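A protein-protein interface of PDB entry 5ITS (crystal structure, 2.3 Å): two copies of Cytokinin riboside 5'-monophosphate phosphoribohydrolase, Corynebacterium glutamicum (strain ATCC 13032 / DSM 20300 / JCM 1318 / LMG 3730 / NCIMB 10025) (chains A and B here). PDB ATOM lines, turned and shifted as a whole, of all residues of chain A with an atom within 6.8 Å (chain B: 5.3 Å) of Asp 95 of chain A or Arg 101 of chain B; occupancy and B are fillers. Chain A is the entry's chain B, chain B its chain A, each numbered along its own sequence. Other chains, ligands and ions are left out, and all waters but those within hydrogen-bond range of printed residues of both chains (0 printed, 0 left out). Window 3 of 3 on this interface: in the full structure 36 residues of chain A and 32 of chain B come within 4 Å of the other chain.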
ATOM      1  N   VAL A  72      17.660 -26.592   2.114  1.00  0.00           N
ATOM      2  CA  VAL A  72      18.002 -25.875   3.318  1.00  0.00           C
ATOM      3  C   VAL A  72      17.962 -26.926   4.366  1.00  0.00           C
ATOM      4  O   VAL A  72      16.962 -27.640   4.500  1.00  0.00           O
ATOM      5  CB  VAL A  72      16.949 -24.832   3.682  1.00  0.00           C
ATOM      6  CG1 VAL A  72      17.358 -24.107   4.958  1.00  0.00           C
ATOM      7  CG2 VAL A  72      16.714 -23.862   2.523  1.00  0.00           C
ATOM      8  N   ILE A  73      19.048 -27.018   5.107  1.00  0.00           N
ATOM      9  CA  ILE A  73      19.308 -28.140   5.959  1.00  0.00           C
ATOM     10  C   ILE A  73      20.019 -27.620   7.201  1.00  0.00           C
ATOM     11  O   ILE A  73      20.526 -26.523   7.169  1.00  0.00           O
ATOM     12  CB  ILE A  73      20.142 -29.153   5.171  1.00  0.00           C
ATOM     13  CG1 ILE A  73      20.123 -30.487   5.866  1.00  0.00           C
ATOM     14  CG2 ILE A  73      21.582 -28.691   5.012  1.00  0.00           C
ATOM     15  CD1 ILE A  73      19.792 -31.625   4.934  1.00  0.00           C
ATOM     16  N   THR A  74      20.025 -28.367   8.298  1.00  0.00           N
ATOM     17  CA  THR A  74      20.639 -27.891   9.536  1.00  0.00           C
ATOM     18  C   THR A  74      22.067 -28.409   9.734  1.00  0.00           C
ATOM     19  O   THR A  74      22.487 -29.347   9.046  1.00  0.00           O
ATOM     20  CB  THR A  74      19.850 -28.329  10.768  1.00  0.00           C
ATOM     21  OG1 THR A  74      19.924 -29.747  10.886  1.00  0.00           O
ATOM     22  CG2 THR A  74      18.423 -27.919  10.648  1.00  0.00           C
ATOM     23  N   GLU A  75      22.785 -27.811  10.690  1.00  0.00           N
ATOM     24  CA  GLU A  75      24.122 -28.291  11.058  1.00  0.00           C
ATOM     25  C   GLU A  75      24.046 -29.722  11.536  1.00  0.00           C
ATOM     26  O   GLU A  75      24.775 -30.571  11.046  1.00  0.00           O
ATOM     27  CB  GLU A  75      24.787 -27.395  12.110  1.00  0.00           C
ATOM     28  CG  GLU A  75      25.406 -26.149  11.472  1.00  0.00           C
ATOM     29  CD  GLU A  75      25.570 -24.980  12.433  1.00  0.00           C
ATOM     30  OE1 GLU A  75      25.756 -25.245  13.639  1.00  0.00           O
ATOM     31  OE2 GLU A  75      25.513 -23.799  11.990  1.00  0.00           O
ATOM     32  N   SER A  76      23.124 -29.986  12.452  1.00  0.00           N
ATOM     33  CA  SER A  76      22.913 -31.331  12.988  1.00  0.00           C
ATOM     34  C   SER A  76      22.789 -32.353  11.856  1.00  0.00           C
ATOM     35  O   SER A  76      23.455 -33.375  11.881  1.00  0.00           O
ATOM     36  CB  SER A  76      21.656 -31.404  13.891  1.00  0.00           C
ATOM     37  OG  SER A  76      21.541 -30.309  14.809  1.00  0.00           O
ATOM     38  N   VAL A  93      22.002 -24.178   8.040  1.00  0.00           N
ATOM     39  CA  VAL A  93      21.563 -23.205   9.065  1.00  0.00           C
ATOM     40  C   VAL A  93      21.562 -23.821  10.473  1.00  0.00           C
ATOM     41  O   VAL A  93      21.419 -25.016  10.615  1.00  0.00           O
ATOM     42  CB  VAL A  93      20.172 -22.632   8.740  1.00  0.00           C
ATOM     43  CG1 VAL A  93      20.171 -22.039   7.357  1.00  0.00           C
ATOM     44  CG2 VAL A  93      19.068 -23.690   8.855  1.00  0.00           C
ATOM     45  N   PRO A  94      21.706 -23.000  11.527  1.00  0.00           N
ATOM     46  CA  PRO A  94      21.915 -23.572  12.870  1.00  0.00           C
ATOM     47  C   PRO A  94      20.794 -24.426  13.488  1.00  0.00           C
ATOM     48  O   PRO A  94      21.101 -25.210  14.406  1.00  0.00           O
ATOM     49  CB  PRO A  94      22.147 -22.340  13.771  1.00  0.00           C
ATOM     50  CG  PRO A  94      22.280 -21.156  12.878  1.00  0.00           C
ATOM     51  CD  PRO A  94      21.726 -21.523  11.525  1.00  0.00           C
ATOM     52  N   ASP A  95      19.532 -24.273  13.044  1.00  0.00           N
ATOM     53  CA  ASP A  95      18.449 -25.057  13.657  1.00  0.00           C
ATOM     54  C   ASP A  95      17.193 -25.203  12.812  1.00  0.00           C
ATOM     55  O   ASP A  95      17.120 -24.709  11.701  1.00  0.00           O
ATOM     56  CB  ASP A  95      18.088 -24.503  15.054  1.00  0.00           C
ATOM     57  CG  ASP A  95      17.434 -23.143  14.980  1.00  0.00           C
ATOM     58  OD1 ASP A  95      16.412 -23.042  14.280  1.00  0.00           O
ATOM     59  OD2 ASP A  95      17.937 -22.179  15.591  1.00  0.00           O
ATOM     60  N   MET A  96      16.209 -25.904  13.357  1.00  0.00           N
ATOM     61  CA  MET A  96      15.043 -26.324  12.602  1.00  0.00           C
ATOM     62  C   MET A  96      14.075 -25.203  12.372  1.00  0.00           C
ATOM     63  O   MET A  96      13.355 -25.202  11.365  1.00  0.00           O
ATOM     64  CB  MET A  96      14.318 -27.426  13.338  1.00  0.00           C
ATOM     65  CG  MET A  96      15.155 -28.662  13.643  1.00  0.00           C
ATOM     66  SD  MET A  96      14.375 -30.130  12.957  1.00  0.00           S
ATOM     67  CE  MET A  96      14.543 -29.653  11.249  1.00  0.00           C
ATOM     68  N   HIS A  97      14.043 -24.265  13.319  1.00  0.00           N
ATOM     69  CA  HIS A  97      13.305 -23.007  13.137  1.00  0.00           C
ATOM     70  C   HIS A  97      13.803 -22.200  11.955  1.00  0.00           C
ATOM     71  O   HIS A  97      13.016 -21.849  11.071  1.00  0.00           O
ATOM     72  CB  HIS A  97      13.346 -22.130  14.402  1.00  0.00           C
ATOM     73  CG  HIS A  97      12.410 -22.577  15.457  1.00  0.00           C
ATOM     74  ND1 HIS A  97      11.227 -23.216  15.168  1.00  0.00           N
ATOM     75  CD2 HIS A  97      12.461 -22.470  16.805  1.00  0.00           C
ATOM     76  CE1 HIS A  97      10.578 -23.468  16.289  1.00  0.00           C
ATOM     77  NE2 HIS A  97      11.312 -23.045  17.298  1.00  0.00           N
ATOM     78  N   ILE A  98      15.095 -21.889  11.942  1.00  0.00           N
ATOM     79  CA  ILE A  98      15.658 -21.067  10.877  1.00  0.00           C
ATOM     80  C   ILE A  98      15.448 -21.791   9.564  1.00  0.00           C
ATOM     81  O   ILE A  98      15.131 -21.160   8.563  1.00  0.00           O
ATOM     82  CB  ILE A  98      17.166 -20.716  11.047  1.00  0.00           C
ATOM     83  CG1 ILE A  98      17.398 -19.909  12.339  1.00  0.00           C
ATOM     84  CG2 ILE A  98      17.615 -19.859   9.879  1.00  0.00           C
ATOM     85  CD1 ILE A  98      18.814 -19.948  12.887  1.00  0.00           C
ATOM     86  N   ARG A  99      15.597 -23.112   9.577  1.00  0.00           N
ATOM     87  CA  ARG A  99      15.371 -23.912   8.375  1.00  0.00           C
ATOM     88  C   ARG A  99      13.996 -23.675   7.796  1.00  0.00           C
ATOM     89  O   ARG A  99      13.870 -23.408   6.626  1.00  0.00           O
ATOM     90  CB  ARG A  99      15.503 -25.377   8.681  1.00  0.00           C
ATOM     91  CG  ARG A  99      15.556 -26.227   7.437  1.00  0.00           C
ATOM     92  CD  ARG A  99      15.044 -27.608   7.719  1.00  0.00           C
ATOM     93  NE  ARG A  99      15.546 -28.650   6.824  1.00  0.00           N
ATOM     94  CZ  ARG A  99      15.102 -29.897   6.897  1.00  0.00           C
ATOM     95  NH1 ARG A  99      14.191 -30.206   7.798  1.00  0.00           N
ATOM     96  NH2 ARG A  99      15.565 -30.841   6.105  1.00  0.00           N
ATOM     97  N   LYS A 100      12.968 -23.776   8.627  1.00  0.00           N
ATOM     98  CA  LYS A 100      11.599 -23.506   8.181  1.00  0.00           C
ATOM     99  C   LYS A 100      11.387 -22.064   7.771  1.00  0.00           C
ATOM    100  O   LYS A 100      10.631 -21.794   6.820  1.00  0.00           O
ATOM    101  CB  LYS A 100      10.554 -23.881   9.270  1.00  0.00           C
ATOM    102  CG  LYS A 100      10.361 -25.383   9.510  1.00  0.00           C
ATOM    103  CD  LYS A 100       9.208 -25.712  10.429  1.00  0.00           C
ATOM    104  CE  LYS A 100       9.545 -25.330  11.849  1.00  0.00           C
ATOM    105  NZ  LYS A 100       8.422 -25.699  12.767  1.00  0.00           N
ATOM    106  N   MET B  96       7.549 -15.717  16.320  1.00  0.00           N
ATOM    107  CA  MET B  96       6.799 -16.925  16.607  1.00  0.00           C
ATOM    108  C   MET B  96       7.755 -18.068  16.971  1.00  0.00           C
ATOM    109  O   MET B  96       7.445 -18.930  17.792  1.00  0.00           O
ATOM    110  CB  MET B  96       6.017 -17.340  15.371  1.00  0.00           C
ATOM    111  CG  MET B  96       4.999 -16.365  14.903  1.00  0.00           C
ATOM    112  SD  MET B  96       3.540 -16.557  15.917  1.00  0.00           S
ATOM    113  CE  MET B  96       2.596 -17.693  14.918  1.00  0.00           C
ATOM    114  N   HIS B  97       8.886 -18.098  16.295  1.00  0.00           N
ATOM    115  CA  HIS B  97       9.857 -19.151  16.515  1.00  0.00           C
ATOM    116  C   HIS B  97      10.524 -19.002  17.863  1.00  0.00           C
ATOM    117  O   HIS B  97      10.700 -20.004  18.571  1.00  0.00           O
ATOM    118  CB  HIS B  97      10.893 -19.196  15.384  1.00  0.00           C
ATOM    119  CG  HIS B  97      10.388 -19.835  14.143  1.00  0.00           C
ATOM    120  ND1 HIS B  97      11.080 -19.801  12.952  1.00  0.00           N
ATOM    121  CD2 HIS B  97       9.251 -20.518  13.894  1.00  0.00           C
ATOM    122  CE1 HIS B  97      10.390 -20.448  12.028  1.00  0.00           C
ATOM    123  NE2 HIS B  97       9.286 -20.906  12.580  1.00  0.00           N
ATOM    124  N   ILE B  98      10.858 -17.783  18.275  1.00  0.00           N
ATOM    125  CA  ILE B  98      11.497 -17.652  19.619  1.00  0.00           C
ATOM    126  C   ILE B  98      10.486 -18.026  20.691  1.00  0.00           C
ATOM    127  O   ILE B  98      10.823 -18.582  21.753  1.00  0.00           O
ATOM    128  CB  ILE B  98      12.116 -16.267  19.865  1.00  0.00           C
ATOM    129  CG1 ILE B  98      13.326 -16.098  18.951  1.00  0.00           C
ATOM    130  CG2 ILE B  98      12.556 -16.098  21.316  1.00  0.00           C
ATOM    131  CD1 ILE B  98      13.709 -14.660  18.701  1.00  0.00           C
ATOM    132  N   ARG B  99       9.239 -17.752  20.369  1.00  0.00           N
ATOM    133  CA  ARG B  99       8.136 -18.035  21.261  1.00  0.00           C
ATOM    134  C   ARG B  99       7.988 -19.537  21.442  1.00  0.00           C
ATOM    135  O   ARG B  99       7.828 -19.973  22.548  1.00  0.00           O
ATOM    136  CB  ARG B  99       6.848 -17.402  20.719  1.00  0.00           C
ATOM    137  CG  ARG B  99       5.544 -17.774  21.424  1.00  0.00           C
ATOM    138  CD  ARG B  99       4.443 -17.093  20.636  1.00  0.00           C
ATOM    139  NE  ARG B  99       3.140 -16.995  21.288  1.00  0.00           N
ATOM    140  CZ  ARG B  99       1.995 -17.331  20.711  1.00  0.00           C
ATOM    141  NH1 ARG B  99       1.972 -17.847  19.502  1.00  0.00           N
ATOM    142  NH2 ARG B  99       0.865 -17.134  21.334  1.00  0.00           N
ATOM    143  N   LYS B 100       8.054 -20.316  20.376  1.00  0.00           N
ATOM    144  CA  LYS B 100       8.017 -21.762  20.534  1.00  0.00           C
ATOM    145  C   LYS B 100       9.299 -22.314  21.169  1.00  0.00           C
ATOM    146  O   LYS B 100       9.192 -23.243  21.964  1.00  0.00           O
ATOM    147  CB  LYS B 100       7.701 -22.458  19.211  1.00  0.00           C
ATOM    148  CG  LYS B 100       6.299 -22.050  18.736  1.00  0.00           C
ATOM    149  CD  LYS B 100       5.794 -22.793  17.523  1.00  0.00           C
ATOM    150  CE  LYS B 100       6.423 -22.257  16.256  1.00  0.00           C
ATOM    151  NZ  LYS B 100       6.467 -23.317  15.202  1.00  0.00           N
ATOM    152  N   ARG B 101      10.483 -21.734  20.882  1.00  0.00           N
ATOM    153  CA  ARG B 101      11.683 -22.186  21.564  1.00  0.00           C
ATOM    154  C   ARG B 101      11.408 -22.018  23.043  1.00  0.00           C
ATOM    155  O   ARG B 101      11.600 -22.952  23.798  1.00  0.00           O
ATOM    156  CB  ARG B 101      12.999 -21.495  21.107  1.00  0.00           C
ATOM    157  CG  ARG B 101      14.281 -22.093  21.735  1.00  0.00           C
ATOM    158  CD  ARG B 101      15.578 -22.018  20.907  1.00  0.00           C
ATOM    159  NE  ARG B 101      15.387 -22.491  19.513  1.00  0.00           N
ATOM    160  CZ  ARG B 101      15.521 -23.757  19.067  1.00  0.00           C
ATOM    161  NH1 ARG B 101      15.895 -24.746  19.888  1.00  0.00           N
ATOM    162  NH2 ARG B 101      15.281 -24.051  17.773  1.00  0.00           N
ATOM    163  N   ARG B 102      10.872 -20.883  23.465  1.00  0.00           N
ATOM    164  CA  ARG B 102      10.729 -20.670  24.902  1.00  0.00           C
ATOM    165  C   ARG B 102       9.657 -21.523  25.558  1.00  0.00           C
ATOM    166  O   ARG B 102       9.809 -21.932  26.710  1.00  0.00           O
ATOM    167  CB  ARG B 102      10.446 -19.213  25.240  1.00  0.00           C
ATOM    168  CG  ARG B 102      11.685 -18.333  25.303  1.00  0.00           C
ATOM    169  CD  ARG B 102      12.617 -18.703  26.470  1.00  0.00           C
ATOM    170  NE  ARG B 102      12.194 -18.212  27.782  1.00  0.00           N
ATOM    171  CZ  ARG B 102      12.619 -18.725  28.936  1.00  0.00           C
ATOM    172  NH1 ARG B 102      12.230 -18.200  30.091  1.00  0.00           N
ATOM    173  NH2 ARG B 102      13.432 -19.785  28.942  1.00  0.00           N
ATOM    174  N   MET B 103       8.549 -21.756  24.874  1.00  0.00           N
ATOM    175  CA  MET B 103       7.507 -22.573  25.463  1.00  0.00           C
ATOM    176  C   MET B 103       8.015 -23.986  25.623  1.00  0.00           C
ATOM    177  O   MET B 103       7.679 -24.665  26.576  1.00  0.00           O
ATOM    178  CB  MET B 103       6.270 -22.548  24.601  1.00  0.00           C
ATOM    179  CG  MET B 103       5.599 -21.182  24.703  1.00  0.00           C
ATOM    180  SD  MET B 103       3.991 -21.125  23.869  1.00  0.00           S
ATOM    181  CE  MET B 103       4.454 -21.451  22.187  1.00  0.00           C
ATOM    182  N   ALA B 104       8.863 -24.421  24.708  1.00  0.00           N
ATOM    183  CA  ALA B 104       9.430 -25.769  24.810  1.00  0.00           C
ATOM    184  C   ALA B 104      10.524 -25.870  25.890  1.00  0.00           C
ATOM    185  O   ALA B 104      10.635 -26.895  26.553  1.00  0.00           O
ATOM    186  CB  ALA B 104       9.916 -26.251  23.460  1.00  0.00           C
ATOM    187  N   GLU B 105      11.290 -24.813  26.100  1.00  0.00           N
ATOM    188  CA  GLU B 105      12.336 -24.835  27.118  1.00  0.00           C
ATOM    189  C   GLU B 105      11.681 -24.902  28.506  1.00  0.00           C
ATOM    190  O   GLU B 105      12.072 -25.708  29.359  1.00  0.00           O
ATOM    191  CB  GLU B 105      13.268 -23.607  26.993  1.00  0.00           C
ATOM    192  CG  GLU B 105      14.192 -23.628  25.746  1.00  0.00           C
ATOM    193  CD  GLU B 105      15.088 -22.377  25.584  1.00  0.00           C
ATOM    194  OE1 GLU B 105      14.978 -21.447  26.435  1.00  0.00           O
ATOM    195  OE2 GLU B 105      15.889 -22.325  24.596  1.00  0.00           O
ATOM    196  N   LEU B 106      10.647 -24.088  28.694  1.00  0.00           N
ATOM    197  CA  LEU B 106       9.968 -23.970  29.961  1.00  0.00           C
ATOM    198  C   LEU B 106       9.094 -25.188  30.289  1.00  0.00           C
ATOM    199  O   LEU B 106       8.907 -25.565  31.453  1.00  0.00           O
ATOM    200  CB  LEU B 106       9.139 -22.691  29.964  1.00  0.00           C
ATOM    201  CG  LEU B 106      10.015 -21.436  30.099  1.00  0.00           C
ATOM    202  CD1 LEU B 106       9.381 -20.177  29.553  1.00  0.00           C
ATOM    203  CD2 LEU B 106      10.322 -21.200  31.542  1.00  0.00           C
ATOM    204  N   TRP B 129       9.666 -33.108  16.829  1.00  0.00           N
ATOM    205  CA  TRP B 129      10.901 -32.977  17.559  1.00  0.00           C
ATOM    206  C   TRP B 129      11.136 -34.049  18.641  1.00  0.00           C
ATOM    207  O   TRP B 129      12.271 -34.338  18.989  1.00  0.00           O
ATOM    208  CB  TRP B 129      10.944 -31.595  18.202  1.00  0.00           C
ATOM    209  CG  TRP B 129      11.099 -30.450  17.254  1.00  0.00           C
ATOM    210  CD1 TRP B 129      10.965 -30.467  15.897  1.00  0.00           C
ATOM    211  CD2 TRP B 129      11.424 -29.119  17.611  1.00  0.00           C
ATOM    212  NE1 TRP B 129      11.163 -29.212  15.387  1.00  0.00           N
ATOM    213  CE2 TRP B 129      11.445 -28.362  16.424  1.00  0.00           C
ATOM    214  CE3 TRP B 129      11.666 -28.480  18.833  1.00  0.00           C
ATOM    215  CZ2 TRP B 129      11.711 -27.007  16.416  1.00  0.00           C
ATOM    216  CZ3 TRP B 129      11.939 -27.147  18.830  1.00  0.00           C
ATOM    217  CH2 TRP B 129      11.962 -26.416  17.623  1.00  0.00           C
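Of the 13 printed residues of chain A, 3 touch a printed residue of chain B.
Hydrophobic or aromatic side chains of chain A within 4 Å of the printed part of chain B: His 97.
Along chain A the printed residues that touch a printed residue of chain B span positions 95 to 100.
Of the 12 printed residues of chain B, 4 touch a printed residue of chain A.
Hydrophobic or aromatic side chains of chain B within 4 Å of the printed part of chain A: His 97 and Trp 129.
Among the printed residues, 5 pairs touch across the chains.
Among the printed residues, Asp or Glu carboxylates within 4 Å of a Lys or Arg side-chain nitrogen of the other chain: Asp 95 of chain A with Arg 101 of chain B (3.8 Å).
The side-chain carboxylate of Asp 95 of chain A sits at hydrogen-bond distance from the backbone NH of Ile 98 of chain A (2.9 Å).
The backbone NH (N) of His 97 of chain A is in hydrogen-bond range of the side-chain carboxylate (OD1) of Asp 95 of chain A, 2.8 Å away.
Among the printed residues, pairs that only touch across the chains: His 97 of chain A with Arg 101 of chain B (3.4 Å), His 97 of chain A with Trp 129 of chain B (3.4 Å) and Lys 100 of chain A with Lys 100 of chain B (3.9 Å).
Asp 95 of chain A touches just one residue of chain B: Arg 101 (3.6 Å).
Of the printed residues of chain B, His 97 of chain A touches His 97, Arg 101 and Trp 129.
Of the printed residues of chain B, Lys 100 of chain A touches Lys 100 (3.9 Å).
Of the printed residues of chain A, His 97 of chain B touches His 97 (3.1 Å).
Of the printed residues of chain A, Lys 100 of chain B touches Lys 100.
The nearest residue of chain A that does not touch Arg 101 of chain B is Met 96 of chain A (4.9 Å).
The side-chain carboxylate (OD1) of Asp 95 of chain A lies within salt-bridge range of the guanidinium group (NH2) of Arg 101 of chain B (3.8 Å).
A ring nitrogen (NE2) of His 97 of chain A is in hydrogen-bond range of the backbone carbonyl oxygen (O) of His 97 of chain B (3.4 Å).
His 97 of chain B touches its own counterpart, His 97 of chain A.
Lys 100 of chain A touches its own counterpart, Lys 100 of chain B.
Positions printed for both chains: 96, 97, 98, 99 and 100.
Of the 5 pairs that touch across the chains among the printed residues, 2 have their exchanged pair printed and touching as well.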
